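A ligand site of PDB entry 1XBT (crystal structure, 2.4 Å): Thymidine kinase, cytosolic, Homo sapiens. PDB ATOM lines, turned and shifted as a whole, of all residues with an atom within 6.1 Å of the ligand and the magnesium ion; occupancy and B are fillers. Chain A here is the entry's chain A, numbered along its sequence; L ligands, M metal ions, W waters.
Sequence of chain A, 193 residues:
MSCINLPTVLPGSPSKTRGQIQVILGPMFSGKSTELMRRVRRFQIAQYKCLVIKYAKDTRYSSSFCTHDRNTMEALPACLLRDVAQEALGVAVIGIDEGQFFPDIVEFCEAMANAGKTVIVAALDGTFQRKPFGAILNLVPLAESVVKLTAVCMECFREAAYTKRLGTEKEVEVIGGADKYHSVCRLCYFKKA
NH2 of Arg 165 is in hydrogen-bond range of OH of Tyr 181. The backbone NH (N) of Met 28 sits at hydrogen-bond distance from the side-chain hydroxyl (OG1) of Thr 163 (3.0 Å). The side-chain hydroxyl of Ser 30 lies within hydrogen-bond range of the backbone carbonyl oxygen of Pro 27. The backbone carbonyl oxygen (O) of Val 172 lies within hydrogen-bond range of the guanidinium group (NH2) of Arg 165 (3.1 Å). OD1 of Asp 58 lies within salt-bridge range of NE of Arg 60 (2.7 Å). NZ of Lys 54 is in salt-bridge range of OE2 of Glu 98 (3.8 Å). N of Gln 129 sits close to OG1 of Thr 127 (3.1 Å). O of Val 174 lies within hydrogen-bond range of OH of Tyr 181.
Water W1 lies within hydrogen-bond range of the side-chain hydroxyl of Ser 33 (2.8 Å), the side-chain carboxylate of Asp 97 (2.9 Å) and an oxygen (O7) of the ligand (3.2 Å). Water W2 lies within hydrogen-bond range of O7 of the ligand (2.8 Å), N of Thr 34 (3.3 Å) and N of Ser 33 (3.4 Å).
The backbone NH (N) of Gly 176 is in hydrogen-bond range of an oxygen (O12) of the ligand (3.2 Å). The side-chain hydroxyl (OG) of Ser 33 lies within hydrogen-bond range of an oxygen (O7) of the ligand (3.1 Å). N2 of the ligand sits at hydrogen-bond distance from O of Val 172 (2.7 Å). O2 of the ligand lies within salt-bridge range of NZ of Lys 32. An oxygen (O9) of the ligand lies within hydrogen-bond range of the backbone NH (N) of Gly 31 (3.1 Å). The backbone NH of Ser 30 lies within hydrogen-bond range of an oxygen (O9) of the ligand (3.5 Å). O of Gly 176 lies close to O12 of the ligand (3.4 Å). The guanidinium group of Arg 60 sits close to an oxygen (O4) of the ligand (3.7 Å). O9 of the ligand lies within hydrogen-bond range of N of Lys 32 (2.8 Å). A nitrogen (N2) of the ligand lies close to the side-chain hydroxyl of Tyr 181 (3.3 Å). O12 of the ligand is in hydrogen-bond range of OD2 of Asp 58, at 2.7 Å. The backbone NH (N) of Ser 33 lies within hydrogen-bond range of an oxygen (O7) of the ligand (3.3 Å). O14 of the ligand lies within hydrogen-bond range of N of Phe 128. The backbone NH of Phe 29 sits at hydrogen-bond distance from an oxygen (O5) of the ligand, 2.9 Å away. An oxygen (O13) of the ligand is in hydrogen-bond range of the backbone NH (N) of Val 174 (2.9 Å).
Merely in contact with the magnesium ion: Ser 33, Arg 60 and Glu 98. Of the 33 residues printed, 3 come within 4 Å of the magnesium ion.
The magnesium ion is bound by an oxygen (O1) of the ligand (2.0 Å) and an oxygen (O4) of the ligand (2.4 Å). The magnesium ion has two donor atoms within binding distance.
Pro 27 touches the ligand. CE of Met 28 touches O3 of the ligand (3.6 Å). CD of Glu 98 touches O10 of the ligand, 3.6 Å away. CZ of Phe 101 touches O11 of the ligand (3.3 Å). Leu 124 touches the ligand. CA of Thr 127 touches O14 of the ligand (3.6 Å). CE1 of Phe 133 touches C7 of the ligand (3.7 Å). CG2 of Thr 163 touches C9 of the ligand (3.8 Å). NH2 of Arg 165 touches N2 of the ligand, 3.5 Å away. Glu 173 touches the ligand. Ile 175 touches the ligand. Hydrophobic or aromatic side chains within 4 Å of the ligand: Met 28, Phe 29, Phe 101, Leu 124, Phe 128, Phe 133, Ile 175 and Tyr 181. Of the 33 residues printed, 23 come within 4 Å of the ligand. The nearest printed residue that does not touch the ligand is Gln 100 (4.03 Å).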
ATOM      1  N   GLY A  26     -21.809 -11.047 -17.619  1.00  0.00           N
ATOM      2  CA  GLY A  26     -20.603 -10.304 -17.270  1.00  0.00           C
ATOM      3  C   GLY A  26     -19.374 -11.164 -17.478  1.00  0.00           C
ATOM      4  O   GLY A  26     -19.496 -12.388 -17.627  1.00  0.00           O
ATOM      5  N   PRO A  27     -18.191 -10.555 -17.452  1.00  0.00           N
ATOM      6  CA  PRO A  27     -16.945 -11.326 -17.555  1.00  0.00           C
ATOM      7  C   PRO A  27     -16.676 -12.003 -16.220  1.00  0.00           C
ATOM      8  O   PRO A  27     -17.489 -11.895 -15.303  1.00  0.00           O
ATOM      9  CB  PRO A  27     -15.899 -10.250 -17.833  1.00  0.00           C
ATOM     10  CG  PRO A  27     -16.446  -9.021 -17.115  1.00  0.00           C
ATOM     11  CD  PRO A  27     -17.941  -9.116 -17.277  1.00  0.00           C
ATOM     12  N   MET A  28     -15.549 -12.692 -16.105  1.00  0.00           N
ATOM     13  CA  MET A  28     -15.140 -13.247 -14.839  1.00  0.00           C
ATOM     14  C   MET A  28     -14.829 -12.112 -13.855  1.00  0.00           C
ATOM     15  O   MET A  28     -14.497 -10.994 -14.278  1.00  0.00           O
ATOM     16  CB  MET A  28     -13.918 -14.135 -15.038  1.00  0.00           C
ATOM     17  CG  MET A  28     -14.238 -15.465 -15.718  1.00  0.00           C
ATOM     18  SD  MET A  28     -12.851 -16.631 -15.766  1.00  0.00           S
ATOM     19  CE  MET A  28     -12.762 -17.017 -14.022  1.00  0.00           C
ATOM     20  N   PHE A  29     -14.934 -12.410 -12.563  1.00  0.00           N
ATOM     21  CA  PHE A  29     -14.549 -11.484 -11.493  1.00  0.00           C
ATOM     22  C   PHE A  29     -15.446 -10.242 -11.367  1.00  0.00           C
ATOM     23  O   PHE A  29     -15.052  -9.247 -10.759  1.00  0.00           O
ATOM     24  CB  PHE A  29     -13.061 -11.083 -11.580  1.00  0.00           C
ATOM     25  CG  PHE A  29     -12.132 -12.231 -11.964  1.00  0.00           C
ATOM     26  CD1 PHE A  29     -11.472 -12.214 -13.199  1.00  0.00           C
ATOM     27  CD2 PHE A  29     -11.909 -13.288 -11.097  1.00  0.00           C
ATOM     28  CE1 PHE A  29     -10.608 -13.243 -13.550  1.00  0.00           C
ATOM     29  CE2 PHE A  29     -11.053 -14.347 -11.447  1.00  0.00           C
ATOM     30  CZ  PHE A  29     -10.393 -14.327 -12.673  1.00  0.00           C
ATOM     31  N   SER A  30     -16.660 -10.321 -11.925  1.00  0.00           N
ATOM     32  CA  SER A  30     -17.607  -9.208 -11.858  1.00  0.00           C
ATOM     33  C   SER A  30     -18.671  -9.386 -10.777  1.00  0.00           C
ATOM     34  O   SER A  30     -19.513  -8.510 -10.584  1.00  0.00           O
ATOM     35  CB  SER A  30     -18.268  -8.964 -13.207  1.00  0.00           C
ATOM     36  OG  SER A  30     -18.760 -10.165 -13.759  1.00  0.00           O
ATOM     37  N   GLY A  31     -18.645 -10.533 -10.097  1.00  0.00           N
ATOM     38  CA  GLY A  31     -19.566 -10.795  -9.010  1.00  0.00           C
ATOM     39  C   GLY A  31     -20.937 -11.313  -9.416  1.00  0.00           C
ATOM     40  O   GLY A  31     -21.936 -11.065  -8.715  1.00  0.00           O
ATOM     41  N   LYS A  32     -21.000 -12.049 -10.531  1.00  0.00           N
ATOM     42  CA  LYS A  32     -22.245 -12.629 -11.034  1.00  0.00           C
ATOM     43  C   LYS A  32     -22.912 -13.564 -10.019  1.00  0.00           C
ATOM     44  O   LYS A  32     -24.127 -13.476  -9.797  1.00  0.00           O
ATOM     45  CB  LYS A  32     -22.035 -13.366 -12.358  1.00  0.00           C
ATOM     46  CG  LYS A  32     -21.546 -12.472 -13.502  1.00  0.00           C
ATOM     47  CD  LYS A  32     -21.305 -13.278 -14.780  1.00  0.00           C
ATOM     48  CE  LYS A  32     -20.441 -14.504 -14.528  1.00  0.00           C
ATOM     49  NZ  LYS A  32     -18.997 -14.131 -14.518  1.00  0.00           N
ATOM     50  N   SER A  33     -22.120 -14.456  -9.428  1.00  0.00           N
ATOM     51  CA  SER A  33     -22.616 -15.370  -8.404  1.00  0.00           C
ATOM     52  C   SER A  33     -23.129 -14.663  -7.158  1.00  0.00           C
ATOM     53  O   SER A  33     -24.120 -15.087  -6.564  1.00  0.00           O
ATOM     54  CB  SER A  33     -21.537 -16.361  -7.976  1.00  0.00           C
ATOM     55  OG  SER A  33     -21.128 -17.113  -9.097  1.00  0.00           O
ATOM     56  N   THR A  34     -22.437 -13.610  -6.758  1.00  0.00           N
ATOM     57  CA  THR A  34     -22.852 -12.794  -5.618  1.00  0.00           C
ATOM     58  C   THR A  34     -24.173 -12.096  -5.891  1.00  0.00           C
ATOM     59  O   THR A  34     -25.053 -12.106  -5.047  1.00  0.00           O
ATOM     60  CB  THR A  34     -21.754 -11.786  -5.266  1.00  0.00           C
ATOM     61  OG1 THR A  34     -20.595 -12.503  -4.812  1.00  0.00           O
ATOM     62  CG2 THR A  34     -22.140 -10.924  -4.069  1.00  0.00           C
ATOM     63  N   LYS A  54     -25.569 -25.383  -9.201  1.00  0.00           N
ATOM     64  CA  LYS A  54     -24.226 -25.036  -9.638  1.00  0.00           C
ATOM     65  C   LYS A  54     -23.683 -26.136 -10.550  1.00  0.00           C
ATOM     66  O   LYS A  54     -24.067 -27.295 -10.429  1.00  0.00           O
ATOM     67  CB  LYS A  54     -23.310 -24.816  -8.421  1.00  0.00           C
ATOM     68  CG  LYS A  54     -21.839 -24.546  -8.758  1.00  0.00           C
ATOM     69  CD  LYS A  54     -21.123 -23.672  -7.720  1.00  0.00           C
ATOM     70  CE  LYS A  54     -20.159 -22.700  -8.405  1.00  0.00           C
ATOM     71  NZ  LYS A  54     -18.734 -22.935  -8.026  1.00  0.00           N
ATOM     72  N   ASP A  58     -17.132 -27.373 -11.830  1.00  0.00           N
ATOM     73  CA  ASP A  58     -16.394 -26.228 -11.295  1.00  0.00           C
ATOM     74  C   ASP A  58     -16.335 -26.306  -9.758  1.00  0.00           C
ATOM     75  O   ASP A  58     -17.309 -26.007  -9.076  1.00  0.00           O
ATOM     76  CB  ASP A  58     -16.999 -24.895 -11.742  1.00  0.00           C
ATOM     77  CG  ASP A  58     -16.039 -23.711 -11.557  1.00  0.00           C
ATOM     78  OD1 ASP A  58     -15.250 -23.721 -10.584  1.00  0.00           O
ATOM     79  OD2 ASP A  58     -16.008 -22.728 -12.339  1.00  0.00           O
ATOM     80  N   ARG A  60     -13.834 -24.862  -7.524  1.00  0.00           N
ATOM     81  CA  ARG A  60     -12.898 -23.924  -6.888  1.00  0.00           C
ATOM     82  C   ARG A  60     -13.278 -23.529  -5.457  1.00  0.00           C
ATOM     83  O   ARG A  60     -14.360 -23.001  -5.196  1.00  0.00           O
ATOM     84  CB  ARG A  60     -12.728 -22.673  -7.760  1.00  0.00           C
ATOM     85  CG  ARG A  60     -12.062 -22.941  -9.105  1.00  0.00           C
ATOM     86  CD  ARG A  60     -12.272 -21.838 -10.138  1.00  0.00           C
ATOM     87  NE  ARG A  60     -13.689 -21.522 -10.324  1.00  0.00           N
ATOM     88  CZ  ARG A  60     -14.160 -20.302 -10.584  1.00  0.00           C
ATOM     89  NH1 ARG A  60     -13.333 -19.269 -10.702  1.00  0.00           N
ATOM     90  NH2 ARG A  60     -15.464 -20.136 -10.728  1.00  0.00           N
ATOM     91  N   ASP A  97     -26.125 -21.061 -11.350  1.00  0.00           N
ATOM     92  CA  ASP A  97     -24.792 -20.500 -11.427  1.00  0.00           C
ATOM     93  C   ASP A  97     -24.015 -21.124 -12.571  1.00  0.00           C
ATOM     94  O   ASP A  97     -24.063 -22.352 -12.764  1.00  0.00           O
ATOM     95  CB  ASP A  97     -24.047 -20.747 -10.111  1.00  0.00           C
ATOM     96  CG  ASP A  97     -22.856 -19.829  -9.931  1.00  0.00           C
ATOM     97  OD1 ASP A  97     -22.764 -18.799 -10.658  1.00  0.00           O
ATOM     98  OD2 ASP A  97     -21.958 -20.051  -9.086  1.00  0.00           O
ATOM     99  N   GLU A  98     -23.298 -20.282 -13.320  1.00  0.00           N
ATOM    100  CA  GLU A  98     -22.480 -20.710 -14.473  1.00  0.00           C
ATOM    101  C   GLU A  98     -23.325 -21.414 -15.537  1.00  0.00           C
ATOM    102  O   GLU A  98     -23.013 -22.522 -15.994  1.00  0.00           O
ATOM    103  CB  GLU A  98     -21.274 -21.564 -14.023  1.00  0.00           C
ATOM    104  CG  GLU A  98     -20.378 -20.875 -12.987  1.00  0.00           C
ATOM    105  CD  GLU A  98     -19.126 -21.657 -12.639  1.00  0.00           C
ATOM    106  OE1 GLU A  98     -18.632 -22.413 -13.494  1.00  0.00           O
ATOM    107  OE2 GLU A  98     -18.631 -21.521 -11.498  1.00  0.00           O
ATOM    108  N   GLN A 100     -23.748 -21.033 -18.601  1.00  0.00           N
ATOM    109  CA  GLN A 100     -23.089 -21.309 -19.879  1.00  0.00           C
ATOM    110  C   GLN A 100     -22.679 -22.771 -20.083  1.00  0.00           C
ATOM    111  O   GLN A 100     -22.598 -23.235 -21.215  1.00  0.00           O
ATOM    112  CB  GLN A 100     -21.880 -20.381 -20.076  1.00  0.00           C
ATOM    113  CG  GLN A 100     -20.650 -20.726 -19.247  1.00  0.00           C
ATOM    114  CD  GLN A 100     -20.625 -20.030 -17.883  1.00  0.00           C
ATOM    115  OE1 GLN A 100     -21.585 -19.361 -17.506  1.00  0.00           O
ATOM    116  NE2 GLN A 100     -19.528 -20.198 -17.158  1.00  0.00           N
ATOM    117  N   PHE A 101     -22.437 -23.495 -18.986  1.00  0.00           N
ATOM    118  CA  PHE A 101     -21.944 -24.879 -19.061  1.00  0.00           C
ATOM    119  C   PHE A 101     -23.050 -25.932 -19.184  1.00  0.00           C
ATOM    120  O   PHE A 101     -22.752 -27.106 -19.383  1.00  0.00           O
ATOM    121  CB  PHE A 101     -21.060 -25.216 -17.854  1.00  0.00           C
ATOM    122  CG  PHE A 101     -19.727 -24.510 -17.835  1.00  0.00           C
ATOM    123  CD1 PHE A 101     -19.390 -23.654 -16.782  1.00  0.00           C
ATOM    124  CD2 PHE A 101     -18.790 -24.725 -18.855  1.00  0.00           C
ATOM    125  CE1 PHE A 101     -18.136 -23.008 -16.749  1.00  0.00           C
ATOM    126  CE2 PHE A 101     -17.558 -24.086 -18.830  1.00  0.00           C
ATOM    127  CZ  PHE A 101     -17.231 -23.228 -17.777  1.00  0.00           C
ATOM    128  N   ALA A 123     -24.247 -16.088 -15.646  1.00  0.00           N
ATOM    129  CA  ALA A 123     -23.481 -16.695 -16.722  1.00  0.00           C
ATOM    130  C   ALA A 123     -22.529 -15.730 -17.404  1.00  0.00           C
ATOM    131  O   ALA A 123     -22.797 -14.531 -17.534  1.00  0.00           O
ATOM    132  CB  ALA A 123     -24.409 -17.314 -17.772  1.00  0.00           C
ATOM    133  N   LEU A 124     -21.449 -16.289 -17.899  1.00  0.00           N
ATOM    134  CA  LEU A 124     -20.528 -15.650 -18.771  1.00  0.00           C
ATOM    135  C   LEU A 124     -21.243 -15.454 -20.111  1.00  0.00           C
ATOM    136  O   LEU A 124     -21.850 -16.404 -20.613  1.00  0.00           O
ATOM    137  CB  LEU A 124     -19.280 -16.536 -19.034  1.00  0.00           C
ATOM    138  CG  LEU A 124     -17.942 -16.264 -18.336  1.00  0.00           C
ATOM    139  CD1 LEU A 124     -18.142 -15.298 -17.192  1.00  0.00           C
ATOM    140  CD2 LEU A 124     -17.321 -17.561 -17.839  1.00  0.00           C
ATOM    141  N   GLY A 126     -19.464 -14.274 -22.796  1.00  0.00           N
ATOM    142  CA  GLY A 126     -18.406 -14.565 -23.749  1.00  0.00           C
ATOM    143  C   GLY A 126     -17.342 -15.511 -23.241  1.00  0.00           C
ATOM    144  O   GLY A 126     -17.028 -15.536 -22.049  1.00  0.00           O
ATOM    145  N   THR A 127     -16.782 -16.309 -24.158  1.00  0.00           N
ATOM    146  CA  THR A 127     -15.589 -17.097 -23.870  1.00  0.00           C
ATOM    147  C   THR A 127     -14.348 -16.189 -23.858  1.00  0.00           C
ATOM    148  O   THR A 127     -14.450 -14.970 -24.074  1.00  0.00           O
ATOM    149  CB  THR A 127     -15.367 -18.198 -24.945  1.00  0.00           C
ATOM    150  OG1 THR A 127     -15.065 -17.577 -26.199  1.00  0.00           O
ATOM    151  CG2 THR A 127     -16.657 -19.006 -25.205  1.00  0.00           C
ATOM    152  N   PHE A 128     -13.190 -16.816 -23.639  1.00  0.00           N
ATOM    153  CA  PHE A 128     -11.899 -16.143 -23.744  1.00  0.00           C
ATOM    154  C   PHE A 128     -11.621 -15.569 -25.141  1.00  0.00           C
ATOM    155  O   PHE A 128     -10.725 -14.758 -25.297  1.00  0.00           O
ATOM    156  CB  PHE A 128     -10.782 -17.094 -23.268  1.00  0.00           C
ATOM    157  CG  PHE A 128     -10.314 -18.079 -24.317  1.00  0.00           C
ATOM    158  CD1 PHE A 128      -9.131 -17.862 -25.021  1.00  0.00           C
ATOM    159  CD2 PHE A 128     -11.060 -19.223 -24.586  1.00  0.00           C
ATOM    160  CE1 PHE A 128      -8.698 -18.761 -25.983  1.00  0.00           C
ATOM    161  CE2 PHE A 128     -10.637 -20.123 -25.557  1.00  0.00           C
ATOM    162  CZ  PHE A 128      -9.454 -19.903 -26.252  1.00  0.00           C
ATOM    163  N   GLN A 129     -12.407 -15.989 -26.139  1.00  0.00           N
ATOM    164  CA  GLN A 129     -12.287 -15.454 -27.496  1.00  0.00           C
ATOM    165  C   GLN A 129     -13.345 -14.397 -27.820  1.00  0.00           C
ATOM    166  O   GLN A 129     -13.469 -13.944 -28.960  1.00  0.00           O
ATOM    167  CB  GLN A 129     -12.302 -16.580 -28.524  1.00  0.00           C
ATOM    168  CG  GLN A 129     -11.088 -17.501 -28.433  1.00  0.00           C
ATOM    169  CD  GLN A 129     -11.135 -18.654 -29.407  1.00  0.00           C
ATOM    170  OE1 GLN A 129     -10.238 -18.809 -30.236  1.00  0.00           O
ATOM    171  NE2 GLN A 129     -12.185 -19.475 -29.307  1.00  0.00           N
ATOM    172  N   PHE A 133     -20.897 -17.923 -25.417  1.00  0.00           N
ATOM    173  CA  PHE A 133     -20.515 -19.063 -24.620  1.00  0.00           C
ATOM    174  C   PHE A 133     -21.650 -20.068 -24.578  1.00  0.00           C
ATOM    175  O   PHE A 133     -22.617 -19.884 -23.844  1.00  0.00           O
ATOM    176  CB  PHE A 133     -20.146 -18.619 -23.194  1.00  0.00           C
ATOM    177  CG  PHE A 133     -19.178 -19.530 -22.516  1.00  0.00           C
ATOM    178  CD1 PHE A 133     -18.188 -19.014 -21.696  1.00  0.00           C
ATOM    179  CD2 PHE A 133     -19.237 -20.914 -22.693  1.00  0.00           C
ATOM    180  CE1 PHE A 133     -17.279 -19.847 -21.065  1.00  0.00           C
ATOM    181  CE2 PHE A 133     -18.343 -21.764 -22.057  1.00  0.00           C
ATOM    182  CZ  PHE A 133     -17.358 -21.227 -21.244  1.00  0.00           C
ATOM    183  N   THR A 163     -12.998 -11.348 -20.614  1.00  0.00           N
ATOM    184  CA  THR A 163     -12.084 -12.267 -19.942  1.00  0.00           C
ATOM    185  C   THR A 163     -10.974 -12.713 -20.883  1.00  0.00           C
ATOM    186  O   THR A 163     -11.242 -13.234 -21.964  1.00  0.00           O
ATOM    187  CB  THR A 163     -12.853 -13.487 -19.417  1.00  0.00           C
ATOM    188  OG1 THR A 163     -13.995 -13.056 -18.661  1.00  0.00           O
ATOM    189  CG2 THR A 163     -12.000 -14.271 -18.399  1.00  0.00           C
ATOM    190  N   ARG A 165      -7.727 -15.261 -21.434  1.00  0.00           N
ATOM    191  CA  ARG A 165      -7.029 -16.464 -20.952  1.00  0.00           C
ATOM    192  C   ARG A 165      -5.523 -16.209 -20.944  1.00  0.00           C
ATOM    193  O   ARG A 165      -4.967 -15.685 -21.903  1.00  0.00           O
ATOM    194  CB  ARG A 165      -7.338 -17.684 -21.832  1.00  0.00           C
ATOM    195  CG  ARG A 165      -6.495 -18.932 -21.508  1.00  0.00           C
ATOM    196  CD  ARG A 165      -7.020 -20.232 -22.119  1.00  0.00           C
ATOM    197  NE  ARG A 165      -8.355 -20.561 -21.594  1.00  0.00           N
ATOM    198  CZ  ARG A 165      -9.224 -21.353 -22.200  1.00  0.00           C
ATOM    199  NH1 ARG A 165      -8.922 -21.934 -23.359  1.00  0.00           N
ATOM    200  NH2 ARG A 165     -10.406 -21.566 -21.636  1.00  0.00           N
ATOM    201  N   GLU A 171      -9.105 -25.212 -26.039  1.00  0.00           N
ATOM    202  CA  GLU A 171     -10.466 -25.673 -25.774  1.00  0.00           C
ATOM    203  C   GLU A 171     -11.242 -24.622 -24.965  1.00  0.00           C
ATOM    204  O   GLU A 171     -10.648 -23.853 -24.216  1.00  0.00           O
ATOM    205  CB  GLU A 171     -10.479 -27.048 -25.084  1.00  0.00           C
ATOM    206  CG  GLU A 171      -9.811 -27.100 -23.720  1.00  0.00           C
ATOM    207  CD  GLU A 171      -8.355 -27.565 -23.758  1.00  0.00           C
ATOM    208  OE1 GLU A 171      -7.763 -27.617 -24.871  1.00  0.00           O
ATOM    209  OE2 GLU A 171      -7.804 -27.864 -22.674  1.00  0.00           O
ATOM    210  N   VAL A 172     -12.554 -24.579 -25.150  1.00  0.00           N
ATOM    211  CA  VAL A 172     -13.397 -23.585 -24.489  1.00  0.00           C
ATOM    212  C   VAL A 172     -13.458 -23.811 -22.969  1.00  0.00           C
ATOM    213  O   VAL A 172     -13.135 -22.925 -22.203  1.00  0.00           O
ATOM    214  CB  VAL A 172     -14.805 -23.513 -25.119  1.00  0.00           C
ATOM    215  CG1 VAL A 172     -15.708 -22.559 -24.345  1.00  0.00           C
ATOM    216  CG2 VAL A 172     -14.701 -23.064 -26.571  1.00  0.00           C
ATOM    217  N   GLU A 173     -13.843 -25.016 -22.555  1.00  0.00           N
ATOM    218  CA  GLU A 173     -13.940 -25.324 -21.132  1.00  0.00           C
ATOM    219  C   GLU A 173     -12.592 -25.621 -20.473  1.00  0.00           C
ATOM    220  O   GLU A 173     -12.040 -26.715 -20.612  1.00  0.00           O
ATOM    221  CB  GLU A 173     -14.929 -26.458 -20.846  1.00  0.00           C
ATOM    222  CG  GLU A 173     -15.064 -26.774 -19.355  1.00  0.00           C
ATOM    223  CD  GLU A 173     -16.236 -27.685 -19.028  1.00  0.00           C
ATOM    224  OE1 GLU A 173     -16.335 -28.109 -17.861  1.00  0.00           O
ATOM    225  OE2 GLU A 173     -17.044 -27.970 -19.947  1.00  0.00           O
ATOM    226  N   VAL A 174     -12.061 -24.627 -19.761  1.00  0.00           N
ATOM    227  CA  VAL A 174     -10.916 -24.805 -18.875  1.00  0.00           C
ATOM    228  C   VAL A 174     -11.217 -24.096 -17.549  1.00  0.00           C
ATOM    229  O   VAL A 174     -11.248 -22.854 -17.499  1.00  0.00           O
ATOM    230  CB  VAL A 174      -9.555 -24.319 -19.489  1.00  0.00           C
ATOM    231  CG1 VAL A 174      -8.384 -24.716 -18.609  1.00  0.00           C
ATOM    232  CG2 VAL A 174      -9.346 -24.845 -20.900  1.00  0.00           C
ATOM    233  N   ILE A 175     -11.455 -24.891 -16.510  1.00  0.00           N
ATOM    234  CA  ILE A 175     -11.812 -24.397 -15.181  1.00  0.00           C
ATOM    235  C   ILE A 175     -10.594 -23.726 -14.539  1.00  0.00           C
ATOM    236  O   ILE A 175      -9.477 -24.230 -14.619  1.00  0.00           O
ATOM    237  CB  ILE A 175     -12.314 -25.560 -14.268  1.00  0.00           C
ATOM    238  CG1 ILE A 175     -13.539 -26.285 -14.879  1.00  0.00           C
ATOM    239  CG2 ILE A 175     -12.607 -25.074 -12.851  1.00  0.00           C
ATOM    240  CD1 ILE A 175     -14.728 -25.389 -15.259  1.00  0.00           C
ATOM    241  N   GLY A 176     -10.827 -22.585 -13.904  1.00  0.00           N
ATOM    242  CA  GLY A 176      -9.757 -21.845 -13.252  1.00  0.00           C
ATOM    243  C   GLY A 176     -10.189 -20.476 -12.780  1.00  0.00           C
ATOM    244  O   GLY A 176     -11.289 -20.017 -13.110  1.00  0.00           O
ATOM    245  N   GLY A 177      -9.328 -19.829 -12.004  1.00  0.00           N
ATOM    246  CA  GLY A 177      -9.590 -18.503 -11.457  1.00  0.00           C
ATOM    247  C   GLY A 177      -8.595 -17.490 -11.977  1.00  0.00           C
ATOM    248  O   GLY A 177      -8.185 -17.540 -13.139  1.00  0.00           O
ATOM    249  N   TYR A 181      -6.956 -16.694 -15.721  1.00  0.00           N
ATOM    250  CA  TYR A 181      -7.730 -15.678 -16.410  1.00  0.00           C
ATOM    251  C   TYR A 181      -7.564 -14.286 -15.802  1.00  0.00           C
ATOM    252  O   TYR A 181      -7.399 -14.160 -14.586  1.00  0.00           O
ATOM    253  CB  TYR A 181      -9.211 -16.017 -16.357  1.00  0.00           C
ATOM    254  CG  TYR A 181      -9.608 -17.288 -17.057  1.00  0.00           C
ATOM    255  CD1 TYR A 181      -9.800 -18.465 -16.327  1.00  0.00           C
ATOM    256  CD2 TYR A 181      -9.829 -17.314 -18.435  1.00  0.00           C
ATOM    257  CE1 TYR A 181     -10.186 -19.639 -16.967  1.00  0.00           C
ATOM    258  CE2 TYR A 181     -10.226 -18.489 -19.085  1.00  0.00           C
ATOM    259  CZ  TYR A 181     -10.393 -19.646 -18.342  1.00  0.00           C
ATOM    260  OH  TYR A 181     -10.779 -20.814 -18.963  1.00  0.00           O
HETATM  261  P1  LIG L   1     -17.507 -17.502 -13.164  1.00  0.00           P
HETATM  262  O1  LIG L   1     -18.362 -17.756 -11.944  1.00  0.00           O
HETATM  263  O2  LIG L   1     -18.079 -16.795 -14.353  1.00  0.00           O
HETATM  264  O3  LIG L   1     -16.119 -16.792 -12.733  1.00  0.00           O
HETATM  265  P2  LIG L   1     -15.931 -15.849 -11.440  1.00  0.00           P
HETATM  266  O4  LIG L   1     -16.300 -16.563 -10.162  1.00  0.00           O
HETATM  267  O5  LIG L   1     -14.642 -15.068 -11.553  1.00  0.00           O
HETATM  268  O6  LIG L   1     -17.096 -14.815 -11.818  1.00  0.00           O
HETATM  269  P3  LIG L   1     -18.075 -14.085 -10.781  1.00  0.00           P
HETATM  270  O7  LIG L   1     -18.963 -15.148 -10.193  1.00  0.00           O
HETATM  271  O8  LIG L   1     -17.129 -13.421  -9.833  1.00  0.00           O
HETATM  272  O9  LIG L   1     -18.704 -13.150 -11.785  1.00  0.00           O
HETATM  273  O10 LIG L   1     -16.944 -18.933 -13.670  1.00  0.00           O
HETATM  274  C1  LIG L   1     -16.017 -19.000 -14.744  1.00  0.00           C
HETATM  275  C2  LIG L   1     -15.576 -20.435 -15.001  1.00  0.00           C
HETATM  276  O11 LIG L   1     -15.597 -20.653 -16.411  1.00  0.00           O
HETATM  277  C3  LIG L   1     -14.137 -20.637 -14.549  1.00  0.00           C
HETATM  278  O12 LIG L   1     -13.966 -21.932 -13.977  1.00  0.00           O
HETATM  279  C4  LIG L   1     -13.304 -20.555 -15.801  1.00  0.00           C
HETATM  280  C5  LIG L   1     -14.293 -21.018 -16.864  1.00  0.00           C
HETATM  281  N1  LIG L   1     -14.049 -20.479 -18.204  1.00  0.00           N
HETATM  282  C6  LIG L   1     -13.891 -21.376 -19.224  1.00  0.00           C
HETATM  283  O13 LIG L   1     -13.947 -22.599 -18.992  1.00  0.00           O
HETATM  284  N2  LIG L   1     -13.688 -20.971 -20.482  1.00  0.00           N
HETATM  285  C7  LIG L   1     -13.626 -19.673 -20.805  1.00  0.00           C
HETATM  286  O14 LIG L   1     -13.416 -19.345 -21.993  1.00  0.00           O
HETATM  287  C8  LIG L   1     -13.783 -18.670 -19.707  1.00  0.00           C
HETATM  288  C9  LIG L   1     -13.731 -17.199 -19.986  1.00  0.00           C
HETATM  289  C10 LIG L   1     -13.997 -19.149 -18.421  1.00  0.00           C
HETATM  290 MG    MG M   1     -18.206 -18.010  -9.941  1.00  0.00          MG
HETATM  291  O   HOH W   1     -20.781 -17.165 -11.895  1.00  0.00           O
HETATM  292  O   HOH W   2     -19.286 -13.991  -7.614  1.00  0.00           O
